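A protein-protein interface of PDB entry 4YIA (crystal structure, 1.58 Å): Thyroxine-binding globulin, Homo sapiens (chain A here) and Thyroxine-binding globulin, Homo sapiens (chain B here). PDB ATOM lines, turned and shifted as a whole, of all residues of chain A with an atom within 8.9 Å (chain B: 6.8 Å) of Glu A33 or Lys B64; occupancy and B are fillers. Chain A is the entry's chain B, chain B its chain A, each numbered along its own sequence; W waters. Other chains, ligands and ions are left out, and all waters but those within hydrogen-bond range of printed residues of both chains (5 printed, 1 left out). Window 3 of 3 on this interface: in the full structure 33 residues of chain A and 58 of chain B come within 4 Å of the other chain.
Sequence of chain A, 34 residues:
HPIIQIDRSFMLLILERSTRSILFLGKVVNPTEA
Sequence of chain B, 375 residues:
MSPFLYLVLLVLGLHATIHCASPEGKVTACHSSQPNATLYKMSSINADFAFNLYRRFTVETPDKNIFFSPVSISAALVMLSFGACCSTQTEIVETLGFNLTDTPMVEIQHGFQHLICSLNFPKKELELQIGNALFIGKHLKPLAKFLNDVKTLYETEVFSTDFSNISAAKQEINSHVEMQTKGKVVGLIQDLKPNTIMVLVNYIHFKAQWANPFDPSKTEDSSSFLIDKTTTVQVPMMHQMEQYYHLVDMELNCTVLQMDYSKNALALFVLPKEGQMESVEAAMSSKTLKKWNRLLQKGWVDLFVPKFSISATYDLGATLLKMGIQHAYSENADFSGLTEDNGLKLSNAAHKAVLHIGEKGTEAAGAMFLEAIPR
Printed residues of chain A that touch a printed residue of chain B: Gly A26, Lys A27, Val A28, Val A29, Asn A30, Pro A31, Thr A32 and Glu A33.
Hydrophobic or aromatic side chains of chain A within 4 Å of the printed part of chain B: Val A29.
Of the 17 printed residues of chain B, 8 touch a printed residue of chain A.
Hydrophobic or aromatic side chains of chain B within 4 Å of the printed part of chain A: Tyr B54, Ile B66 and Val B233.
Among the printed residues, 16 pairs touch across the chains.
Among the printed residues, Asp or Glu carboxylates within 4 Å of a Lys or Arg side-chain nitrogen of the other chain: Lys A27 with Glu B281 (2.8 Å) and Glu A33 with Lys B64 (3.1 Å).
Printed residues of chain B within 4 Å of Val A28: Asn B65 (3.7 Å).
Glu A33 touches just these residues of chain B: Lys B64 and Asn B65.
Lys B64 touches just these residues of chain A: Lys A27, Val A29 and Glu A33.
Of the printed residues of chain A, Asn B65 touches Lys A27 (3.3 Å), Val A28 (3.7 Å), Val A29 (2.7 Å), Asn A30 (2.9 Å) and Glu A33 (3.6 Å).
Phe B67 touches none of the printed residues of chain A.
Printed residues of chain A within 4 Å of Ser B309: Pro A31 (3.4 Å).
Ile B310 touches none of the printed residues of chain A.
The nearest residue of chain B that does not touch Glu A33 is Ser B309 (4.7 Å).
Water W2 bridges OE1 of Glu B281 (2.6 Å) and NZ of Lys A27 (3.4 Å).
Water W3 lies within hydrogen-bond range of the backbone carbonyl oxygen of Lys B64 (2.7 Å), the backbone carbonyl oxygen of Thr B61 (2.8 Å), the side-chain amino group of Lys A27 (2.9 Å) and the backbone NH of Asp B63 (3.3 Å).
Water W1 bridges O of Pro A31 (2.7 Å) and N of Ser B309 (3.0 Å).
Water W4 bridges NZ of Lys A27 (2.8 Å) and OD1 of Asp B63 (2.8 Å).
Water W5 lies within hydrogen-bond range of the backbone NH of Asp B63, the backbone carbonyl oxygen of Thr B58 and the side-chain amino group of Lys A27.
Ile B66 touches Gly A26 (O to CA, 3.0 Å).
Lys A27 touches Tyr B54.
Lys B64 touches Lys A27 (O to CE, 3.7 Å).
CA of Asn B65 touches O of Lys A27, 3.3 Å away.
OD1 of Asn B65 touches C of Val A28 (3.7 Å).
Asp B63 touches Val A29 (O to CG1, 3.9 Å).
CG2 of Val A29 touches C of Lys B64, 3.7 Å away.
CG2 of Val B233 touches OD1 of Asn A30 (3.7 Å).
Val B233 touches Thr A32 (CB to OG1, 3.8 Å).
Glu A33 touches Asn B65 (OE1 to ND2, 3.6 Å).
The side-chain amino group of Lys B64 is in salt-bridge range of the side-chain carboxylate of Glu A33 (3.1 Å).
The side-chain amide oxygen of Asn B65 is in hydrogen-bond range of the backbone NH of Val A29 (2.7 Å).
The side-chain amide oxygen (OD1) of Asn B65 lies within hydrogen-bond range of the backbone NH (N) of Asn A30, at 2.9 Å.
The backbone carbonyl oxygen of Ile B66 lies within hydrogen-bond range of the backbone NH of Lys A27 (2.8 Å).
The side-chain amino group of Lys A27 is in salt-bridge range of the side-chain carboxylate of Glu B281, 2.8 Å away.
O of Pro A31 lies close to O of Ser B309.
The side-chain carboxylate (OE2) of Glu B281 is in hydrogen-bond range of the side-chain hydroxyl (OH) of Tyr B54 (2.6 Å).
The backbone NH of Val A28 lies within hydrogen-bond range of the backbone carbonyl oxygen of Phe A10 (2.9 Å).
N of Thr A32 sits at hydrogen-bond distance from OD1 of Asn A30, at 3.0 Å.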
ATOM      1  N   SER A   9      11.802 -25.351  23.098  1.00  0.00           N
ATOM      2  CA  SER A   9      12.687 -24.305  22.574  1.00  0.00           C
ATOM      3  C   SER A   9      12.704 -24.293  21.046  1.00  0.00           C
ATOM      4  O   SER A   9      12.754 -25.352  20.401  1.00  0.00           O
ATOM      5  CB  SER A   9      14.119 -24.559  22.985  1.00  0.00           C
ATOM      6  OG  SER A   9      14.256 -24.463  24.382  1.00  0.00           O
ATOM      7  N   PHE A  10      12.697 -23.097  20.493  1.00  0.00           N
ATOM      8  CA  PHE A  10      12.704 -22.924  19.015  1.00  0.00           C
ATOM      9  C   PHE A  10      13.578 -21.760  18.631  1.00  0.00           C
ATOM     10  O   PHE A  10      13.748 -20.846  19.396  1.00  0.00           O
ATOM     11  CB  PHE A  10      11.224 -22.788  18.527  1.00  0.00           C
ATOM     12  CG  PHE A  10      10.479 -21.574  18.973  1.00  0.00           C
ATOM     13  CD1 PHE A  10       9.831 -21.556  20.200  1.00  0.00           C
ATOM     14  CD2 PHE A  10      10.401 -20.421  18.168  1.00  0.00           C
ATOM     15  CE1 PHE A  10       9.038 -20.485  20.595  1.00  0.00           C
ATOM     16  CE2 PHE A  10       9.691 -19.319  18.553  1.00  0.00           C
ATOM     17  CZ  PHE A  10       9.025 -19.332  19.811  1.00  0.00           C
ATOM     18  N   GLY A  26      16.564 -15.115  16.594  1.00  0.00           N
ATOM     19  CA  GLY A  26      16.668 -15.520  17.993  1.00  0.00           C
ATOM     20  C   GLY A  26      16.327 -16.947  18.309  1.00  0.00           C
ATOM     21  O   GLY A  26      16.058 -17.724  17.433  1.00  0.00           O
ATOM     22  N   LYS A  27      16.385 -17.223  19.636  1.00  0.00           N
ATOM     23  CA  LYS A  27      15.987 -18.454  20.244  1.00  0.00           C
ATOM     24  C   LYS A  27      15.186 -18.249  21.431  1.00  0.00           C
ATOM     25  O   LYS A  27      15.557 -17.464  22.281  1.00  0.00           O
ATOM     26  CB  LYS A  27      17.253 -19.307  20.582  1.00  0.00           C
ATOM     27  CG  LYS A  27      16.912 -20.569  21.347  1.00  0.00           C
ATOM     28  CD  LYS A  27      18.097 -21.514  21.602  1.00  0.00           C
ATOM     29  CE  LYS A  27      19.201 -20.885  22.372  1.00  0.00           C
ATOM     30  NZ  LYS A  27      20.330 -21.798  22.685  1.00  0.00           N
ATOM     31  N   VAL A  28      14.050 -18.929  21.496  1.00  0.00           N
ATOM     32  CA  VAL A  28      13.183 -18.789  22.615  1.00  0.00           C
ATOM     33  C   VAL A  28      13.332 -20.075  23.411  1.00  0.00           C
ATOM     34  O   VAL A  28      12.890 -21.140  22.953  1.00  0.00           O
ATOM     35  CB  VAL A  28      11.741 -18.571  22.180  1.00  0.00           C
ATOM     36  CG1 VAL A  28      10.870 -18.463  23.407  1.00  0.00           C
ATOM     37  CG2 VAL A  28      11.578 -17.296  21.393  1.00  0.00           C
ATOM     38  N   VAL A  29      13.889 -19.915  24.602  1.00  0.00           N
ATOM     39  CA  VAL A  29      14.006 -20.996  25.611  1.00  0.00           C
ATOM     40  C   VAL A  29      12.943 -20.921  26.643  1.00  0.00           C
ATOM     41  O   VAL A  29      12.292 -21.917  26.963  1.00  0.00           O
ATOM     42  CB  VAL A  29      15.423 -20.994  26.229  1.00  0.00           C
ATOM     43  CG1 VAL A  29      15.524 -22.129  27.231  1.00  0.00           C
ATOM     44  CG2 VAL A  29      16.571 -21.179  25.188  1.00  0.00           C
ATOM     45  N   ASN A  30      12.680 -19.722  27.109  1.00  0.00           N
ATOM     46  CA  ASN A  30      11.677 -19.472  28.104  1.00  0.00           C
ATOM     47  C   ASN A  30      10.866 -18.253  27.732  1.00  0.00           C
ATOM     48  O   ASN A  30      11.343 -17.105  27.937  1.00  0.00           O
ATOM     49  CB  ASN A  30      12.281 -19.319  29.499  1.00  0.00           C
ATOM     50  CG  ASN A  30      11.216 -19.068  30.549  1.00  0.00           C
ATOM     51  OD1 ASN A  30      10.056 -18.962  30.222  1.00  0.00           O
ATOM     52  ND2 ASN A  30      11.584 -19.037  31.801  1.00  0.00           N
ATOM     53  N   PRO A  31       9.687 -18.437  27.200  1.00  0.00           N
ATOM     54  CA  PRO A  31       8.910 -17.289  26.667  1.00  0.00           C
ATOM     55  C   PRO A  31       8.368 -16.349  27.747  1.00  0.00           C
ATOM     56  O   PRO A  31       7.830 -15.272  27.375  1.00  0.00           O
ATOM     57  CB  PRO A  31       7.802 -17.958  25.897  1.00  0.00           C
ATOM     58  CG  PRO A  31       7.738 -19.360  26.399  1.00  0.00           C
ATOM     59  CD  PRO A  31       9.049 -19.735  26.854  1.00  0.00           C
ATOM     60  N   THR A  32       8.487 -16.735  29.003  1.00  0.00           N
ATOM     61  CA  THR A  32       7.944 -15.859  30.081  1.00  0.00           C
ATOM     62  C   THR A  32       9.073 -15.273  30.916  1.00  0.00           C
ATOM     63  O   THR A  32       8.775 -14.592  31.904  1.00  0.00           O
ATOM     64  CB  THR A  32       6.921 -16.603  30.980  1.00  0.00           C
ATOM     65  OG1 THR A  32       7.614 -17.664  31.608  1.00  0.00           O
ATOM     66  CG2 THR A  32       5.695 -17.185  30.186  1.00  0.00           C
ATOM     67  N   GLU A  33      10.354 -15.440  30.520  1.00  0.00           N
ATOM     68  CA  GLU A  33      11.490 -14.803  31.229  1.00  0.00           C
ATOM     69  C   GLU A  33      11.273 -13.308  31.419  1.00  0.00           C
ATOM     70  O   GLU A  33      11.059 -12.629  30.425  1.00  0.00           O
ATOM     71  CB  GLU A  33      12.794 -15.060  30.470  1.00  0.00           C
ATOM     72  CG  GLU A  33      14.020 -14.268  30.929  1.00  0.00           C
ATOM     73  CD  GLU A  33      15.302 -14.849  30.342  1.00  0.00           C
ATOM     74  OE1 GLU A  33      15.960 -14.247  29.407  1.00  0.00           O
ATOM     75  OE2 GLU A  33      15.622 -15.960  30.803  1.00  0.00           O
ATOM     76  N   TYR B  54      25.107 -15.250  16.265  1.00  0.00           N
ATOM     77  CA  TYR B  54      24.256 -16.118  17.010  1.00  0.00           C
ATOM     78  C   TYR B  54      25.014 -17.166  17.753  1.00  0.00           C
ATOM     79  O   TYR B  54      24.789 -17.372  18.995  1.00  0.00           O
ATOM     80  CB  TYR B  54      23.130 -16.651  16.126  1.00  0.00           C
ATOM     81  CG  TYR B  54      22.266 -17.610  16.830  1.00  0.00           C
ATOM     82  CD1 TYR B  54      22.649 -18.956  16.942  1.00  0.00           C
ATOM     83  CD2 TYR B  54      21.065 -17.207  17.368  1.00  0.00           C
ATOM     84  CE1 TYR B  54      21.853 -19.866  17.614  1.00  0.00           C
ATOM     85  CE2 TYR B  54      20.260 -18.109  18.021  1.00  0.00           C
ATOM     86  CZ  TYR B  54      20.707 -19.419  18.209  1.00  0.00           C
ATOM     87  OH  TYR B  54      19.897 -20.325  18.902  1.00  0.00           O
ATOM     88  N   PHE B  57      26.776 -15.880  20.708  1.00  0.00           N
ATOM     89  CA  PHE B  57      25.849 -15.704  21.825  1.00  0.00           C
ATOM     90  C   PHE B  57      25.422 -16.969  22.506  1.00  0.00           C
ATOM     91  O   PHE B  57      25.223 -16.966  23.763  1.00  0.00           O
ATOM     92  CB  PHE B  57      24.586 -14.945  21.374  1.00  0.00           C
ATOM     93  CG  PHE B  57      24.774 -13.603  20.850  1.00  0.00           C
ATOM     94  CD1 PHE B  57      25.869 -12.795  21.194  1.00  0.00           C
ATOM     95  CD2 PHE B  57      23.876 -13.070  19.941  1.00  0.00           C
ATOM     96  CE1 PHE B  57      25.981 -11.549  20.668  1.00  0.00           C
ATOM     97  CE2 PHE B  57      24.013 -11.821  19.391  1.00  0.00           C
ATOM     98  CZ  PHE B  57      25.077 -11.021  19.755  1.00  0.00           C
ATOM     99  N   THR B  58      25.363 -18.115  21.817  1.00  0.00           N
ATOM    100  CA  THR B  58      24.986 -19.350  22.457  1.00  0.00           C
ATOM    101  C   THR B  58      26.089 -19.841  23.398  1.00  0.00           C
ATOM    102  O   THR B  58      25.824 -20.719  24.289  1.00  0.00           O
ATOM    103  CB  THR B  58      24.681 -20.522  21.500  1.00  0.00           C
ATOM    104  OG1 THR B  58      25.842 -20.878  20.746  1.00  0.00           O
ATOM    105  CG2 THR B  58      23.562 -20.117  20.581  1.00  0.00           C
ATOM    106  N   THR B  61      25.881 -16.847  26.513  1.00  0.00           N
ATOM    107  CA  THR B  61      24.657 -17.008  27.334  1.00  0.00           C
ATOM    108  C   THR B  61      24.042 -18.344  26.980  1.00  0.00           C
ATOM    109  O   THR B  61      23.080 -18.455  26.199  1.00  0.00           O
ATOM    110  CB  THR B  61      23.625 -15.854  27.122  1.00  0.00           C
ATOM    111  OG1 THR B  61      23.361 -15.700  25.729  1.00  0.00           O
ATOM    112  CG2 THR B  61      24.185 -14.546  27.518  1.00  0.00           C
ATOM    113  N   PRO B  62      24.621 -19.456  27.458  1.00  0.00           N
ATOM    114  CA  PRO B  62      24.176 -20.798  27.065  1.00  0.00           C
ATOM    115  C   PRO B  62      22.820 -21.145  27.609  1.00  0.00           C
ATOM    116  O   PRO B  62      22.493 -20.832  28.786  1.00  0.00           O
ATOM    117  CB  PRO B  62      25.276 -21.702  27.631  1.00  0.00           C
ATOM    118  CG  PRO B  62      25.809 -20.926  28.797  1.00  0.00           C
ATOM    119  CD  PRO B  62      25.760 -19.489  28.372  1.00  0.00           C
ATOM    120  N   ASP B  63      21.985 -21.751  26.780  1.00  0.00           N
ATOM    121  CA  ASP B  63      20.636 -22.216  27.165  1.00  0.00           C
ATOM    122  C   ASP B  63      19.787 -21.070  27.731  1.00  0.00           C
ATOM    123  O   ASP B  63      19.002 -21.233  28.693  1.00  0.00           O
ATOM    124  CB  ASP B  63      20.666 -23.451  28.126  1.00  0.00           C
ATOM    125  CG  ASP B  63      21.280 -24.652  27.473  1.00  0.00           C
ATOM    126  OD1 ASP B  63      21.134 -24.806  26.231  1.00  0.00           O
ATOM    127  OD2 ASP B  63      21.926 -25.452  28.181  1.00  0.00           O
ATOM    128  N   LYS B  64      19.951 -19.927  27.102  1.00  0.00           N
ATOM    129  CA  LYS B  64      19.188 -18.719  27.422  1.00  0.00           C
ATOM    130  C   LYS B  64      18.531 -18.146  26.165  1.00  0.00           C
ATOM    131  O   LYS B  64      19.026 -18.346  25.075  1.00  0.00           O
ATOM    132  CB  LYS B  64      20.124 -17.636  28.006  1.00  0.00           C
ATOM    133  CG  LYS B  64      20.747 -18.062  29.355  1.00  0.00           C
ATOM    134  CD  LYS B  64      19.698 -18.092  30.458  1.00  0.00           C
ATOM    135  CE  LYS B  64      19.159 -16.729  30.798  1.00  0.00           C
ATOM    136  NZ  LYS B  64      18.379 -16.815  32.048  1.00  0.00           N
ATOM    137  N   ASN B  65      17.423 -17.425  26.330  1.00  0.00           N
ATOM    138  CA  ASN B  65      16.859 -16.699  25.198  1.00  0.00           C
ATOM    139  C   ASN B  65      17.898 -15.830  24.523  1.00  0.00           C
ATOM    140  O   ASN B  65      18.732 -15.176  25.205  1.00  0.00           O
ATOM    141  CB  ASN B  65      15.745 -15.739  25.663  1.00  0.00           C
ATOM    142  CG  ASN B  65      14.512 -16.449  26.224  1.00  0.00           C
ATOM    143  OD1 ASN B  65      14.227 -17.588  25.966  1.00  0.00           O
ATOM    144  ND2 ASN B  65      13.702 -15.682  26.985  1.00  0.00           N
ATOM    145  N   ILE B  66      17.832 -15.785  23.172  1.00  0.00           N
ATOM    146  CA  ILE B  66      18.682 -14.973  22.319  1.00  0.00           C
ATOM    147  C   ILE B  66      17.745 -14.175  21.433  1.00  0.00           C
ATOM    148  O   ILE B  66      16.759 -14.730  20.926  1.00  0.00           O
ATOM    149  CB  ILE B  66      19.599 -15.811  21.418  1.00  0.00           C
ATOM    150  CG1 ILE B  66      20.628 -16.520  22.307  1.00  0.00           C
ATOM    151  CG2 ILE B  66      20.292 -14.937  20.373  1.00  0.00           C
ATOM    152  CD1 ILE B  66      21.592 -17.523  21.710  1.00  0.00           C
ATOM    153  N   PHE B  67      17.941 -12.864  21.319  1.00  0.00           N
ATOM    154  CA  PHE B  67      17.177 -12.117  20.382  1.00  0.00           C
ATOM    155  C   PHE B  67      17.934 -10.856  19.990  1.00  0.00           C
ATOM    156  O   PHE B  67      18.319 -10.067  20.847  1.00  0.00           O
ATOM    157  CB  PHE B  67      15.776 -11.664  20.932  1.00  0.00           C
ATOM    158  CG  PHE B  67      14.848 -11.105  19.859  1.00  0.00           C
ATOM    159  CD1 PHE B  67      14.315 -11.945  18.869  1.00  0.00           C
ATOM    160  CD2 PHE B  67      14.575  -9.771  19.770  1.00  0.00           C
ATOM    161  CE1 PHE B  67      13.659 -11.467  17.775  1.00  0.00           C
ATOM    162  CE2 PHE B  67      13.741  -9.289  18.727  1.00  0.00           C
ATOM    163  CZ  PHE B  67      13.281 -10.128  17.740  1.00  0.00           C
ATOM    164  N   VAL B 233       6.770 -23.930  31.786  1.00  0.00           N
ATOM    165  CA  VAL B 233       6.092 -22.702  32.137  1.00  0.00           C
ATOM    166  C   VAL B 233       4.769 -22.568  31.413  1.00  0.00           C
ATOM    167  O   VAL B 233       4.488 -23.246  30.427  1.00  0.00           O
ATOM    168  CB  VAL B 233       6.977 -21.442  31.848  1.00  0.00           C
ATOM    169  CG1 VAL B 233       8.302 -21.589  32.519  1.00  0.00           C
ATOM    170  CG2 VAL B 233       7.134 -21.291  30.309  1.00  0.00           C
ATOM    171  N   GLU B 281      21.630 -25.524  15.640  1.00  0.00           N
ATOM    172  CA  GLU B 281      22.408 -24.273  15.795  1.00  0.00           C
ATOM    173  C   GLU B 281      23.721 -24.350  15.035  1.00  0.00           C
ATOM    174  O   GLU B 281      24.140 -23.391  14.434  1.00  0.00           O
ATOM    175  CB  GLU B 281      22.689 -23.971  17.243  1.00  0.00           C
ATOM    176  CG  GLU B 281      21.415 -23.580  17.977  1.00  0.00           C
ATOM    177  CD  GLU B 281      21.586 -23.365  19.480  1.00  0.00           C
ATOM    178  OE1 GLU B 281      22.318 -24.151  20.098  1.00  0.00           O
ATOM    179  OE2 GLU B 281      20.973 -22.380  20.052  1.00  0.00           O
ATOM    180  N   SER B 309       6.327 -12.184  24.894  1.00  0.00           N
ATOM    181  CA  SER B 309       7.255 -11.086  24.685  1.00  0.00           C
ATOM    182  C   SER B 309       8.580 -11.489  25.307  1.00  0.00           C
ATOM    183  O   SER B 309       8.562 -12.114  26.426  1.00  0.00           O
ATOM    184  CB  SER B 309       6.780  -9.825  25.336  1.00  0.00           C
ATOM    185  OG  SER B 309       5.589  -9.400  24.790  1.00  0.00           O
ATOM    186  N   ILE B 310       9.673 -11.120  24.667  1.00  0.00           N
ATOM    187  CA  ILE B 310      10.974 -11.260  25.289  1.00  0.00           C
ATOM    188  C   ILE B 310      11.884 -10.068  24.898  1.00  0.00           C
ATOM    189  O   ILE B 310      11.584  -9.262  24.026  1.00  0.00           O
ATOM    190  CB  ILE B 310      11.701 -12.535  24.929  1.00  0.00           C
ATOM    191  CG1 ILE B 310      11.992 -12.655  23.445  1.00  0.00           C
ATOM    192  CG2 ILE B 310      10.966 -13.752  25.388  1.00  0.00           C
ATOM    193  CD1 ILE B 310      12.990 -13.758  23.020  1.00  0.00           C
ATOM    194  N   SER B 311      12.957  -9.955  25.655  1.00  0.00           N
ATOM    195  CA  SER B 311      13.980  -8.887  25.378  1.00  0.00           C
ATOM    196  C   SER B 311      15.348  -9.432  25.655  1.00  0.00           C
ATOM    197  O   SER B 311      15.496 -10.352  26.494  1.00  0.00           O
ATOM    198  CB  SER B 311      13.626  -7.660  26.125  1.00  0.00           C
ATOM    199  OG  SER B 311      13.857  -7.888  27.435  1.00  0.00           O
ATOM    200  N   ALA B 312      16.383  -8.862  25.012  1.00  0.00           N
ATOM    201  CA  ALA B 312      17.696  -9.266  25.262  1.00  0.00           C
ATOM    202  C   ALA B 312      18.677  -8.106  25.069  1.00  0.00           C
ATOM    203  O   ALA B 312      18.402  -7.183  24.303  1.00  0.00           O
ATOM    204  CB  ALA B 312      18.075 -10.432  24.388  1.00  0.00           C
ATOM    205  N   TYR B 314      23.037  -7.180  24.839  1.00  0.00           N
ATOM    206  CA  TYR B 314      24.387  -7.711  24.559  1.00  0.00           C
ATOM    207  C   TYR B 314      25.409  -6.589  24.740  1.00  0.00           C
ATOM    208  O   TYR B 314      25.255  -5.513  24.191  1.00  0.00           O
ATOM    209  CB  TYR B 314      24.479  -8.224  23.105  1.00  0.00           C
ATOM    210  CG  TYR B 314      23.504  -9.334  22.886  1.00  0.00           C
ATOM    211  CD1 TYR B 314      23.758 -10.588  23.331  1.00  0.00           C
ATOM    212  CD2 TYR B 314      22.255  -9.072  22.461  1.00  0.00           C
ATOM    213  CE1 TYR B 314      22.791 -11.585  23.287  1.00  0.00           C
ATOM    214  CE2 TYR B 314      21.315 -10.093  22.305  1.00  0.00           C
ATOM    215  CZ  TYR B 314      21.607 -11.350  22.766  1.00  0.00           C
ATOM    216  OH  TYR B 314      20.624 -12.332  22.787  1.00  0.00           O
HETATM  217  O   HOH W   1       5.762 -13.511  27.571  1.00  0.00           O
HETATM  218  O   HOH W   2      22.133 -24.698  22.595  1.00  0.00           O
HETATM  219  O   HOH W   3      21.310 -19.619  24.327  1.00  0.00           O
HETATM  220  O   HOH W   4      19.389 -23.801  24.331  1.00  0.00           O
HETATM  221  O   HOH W   5      23.117 -22.430  24.219  1.00  0.00           O
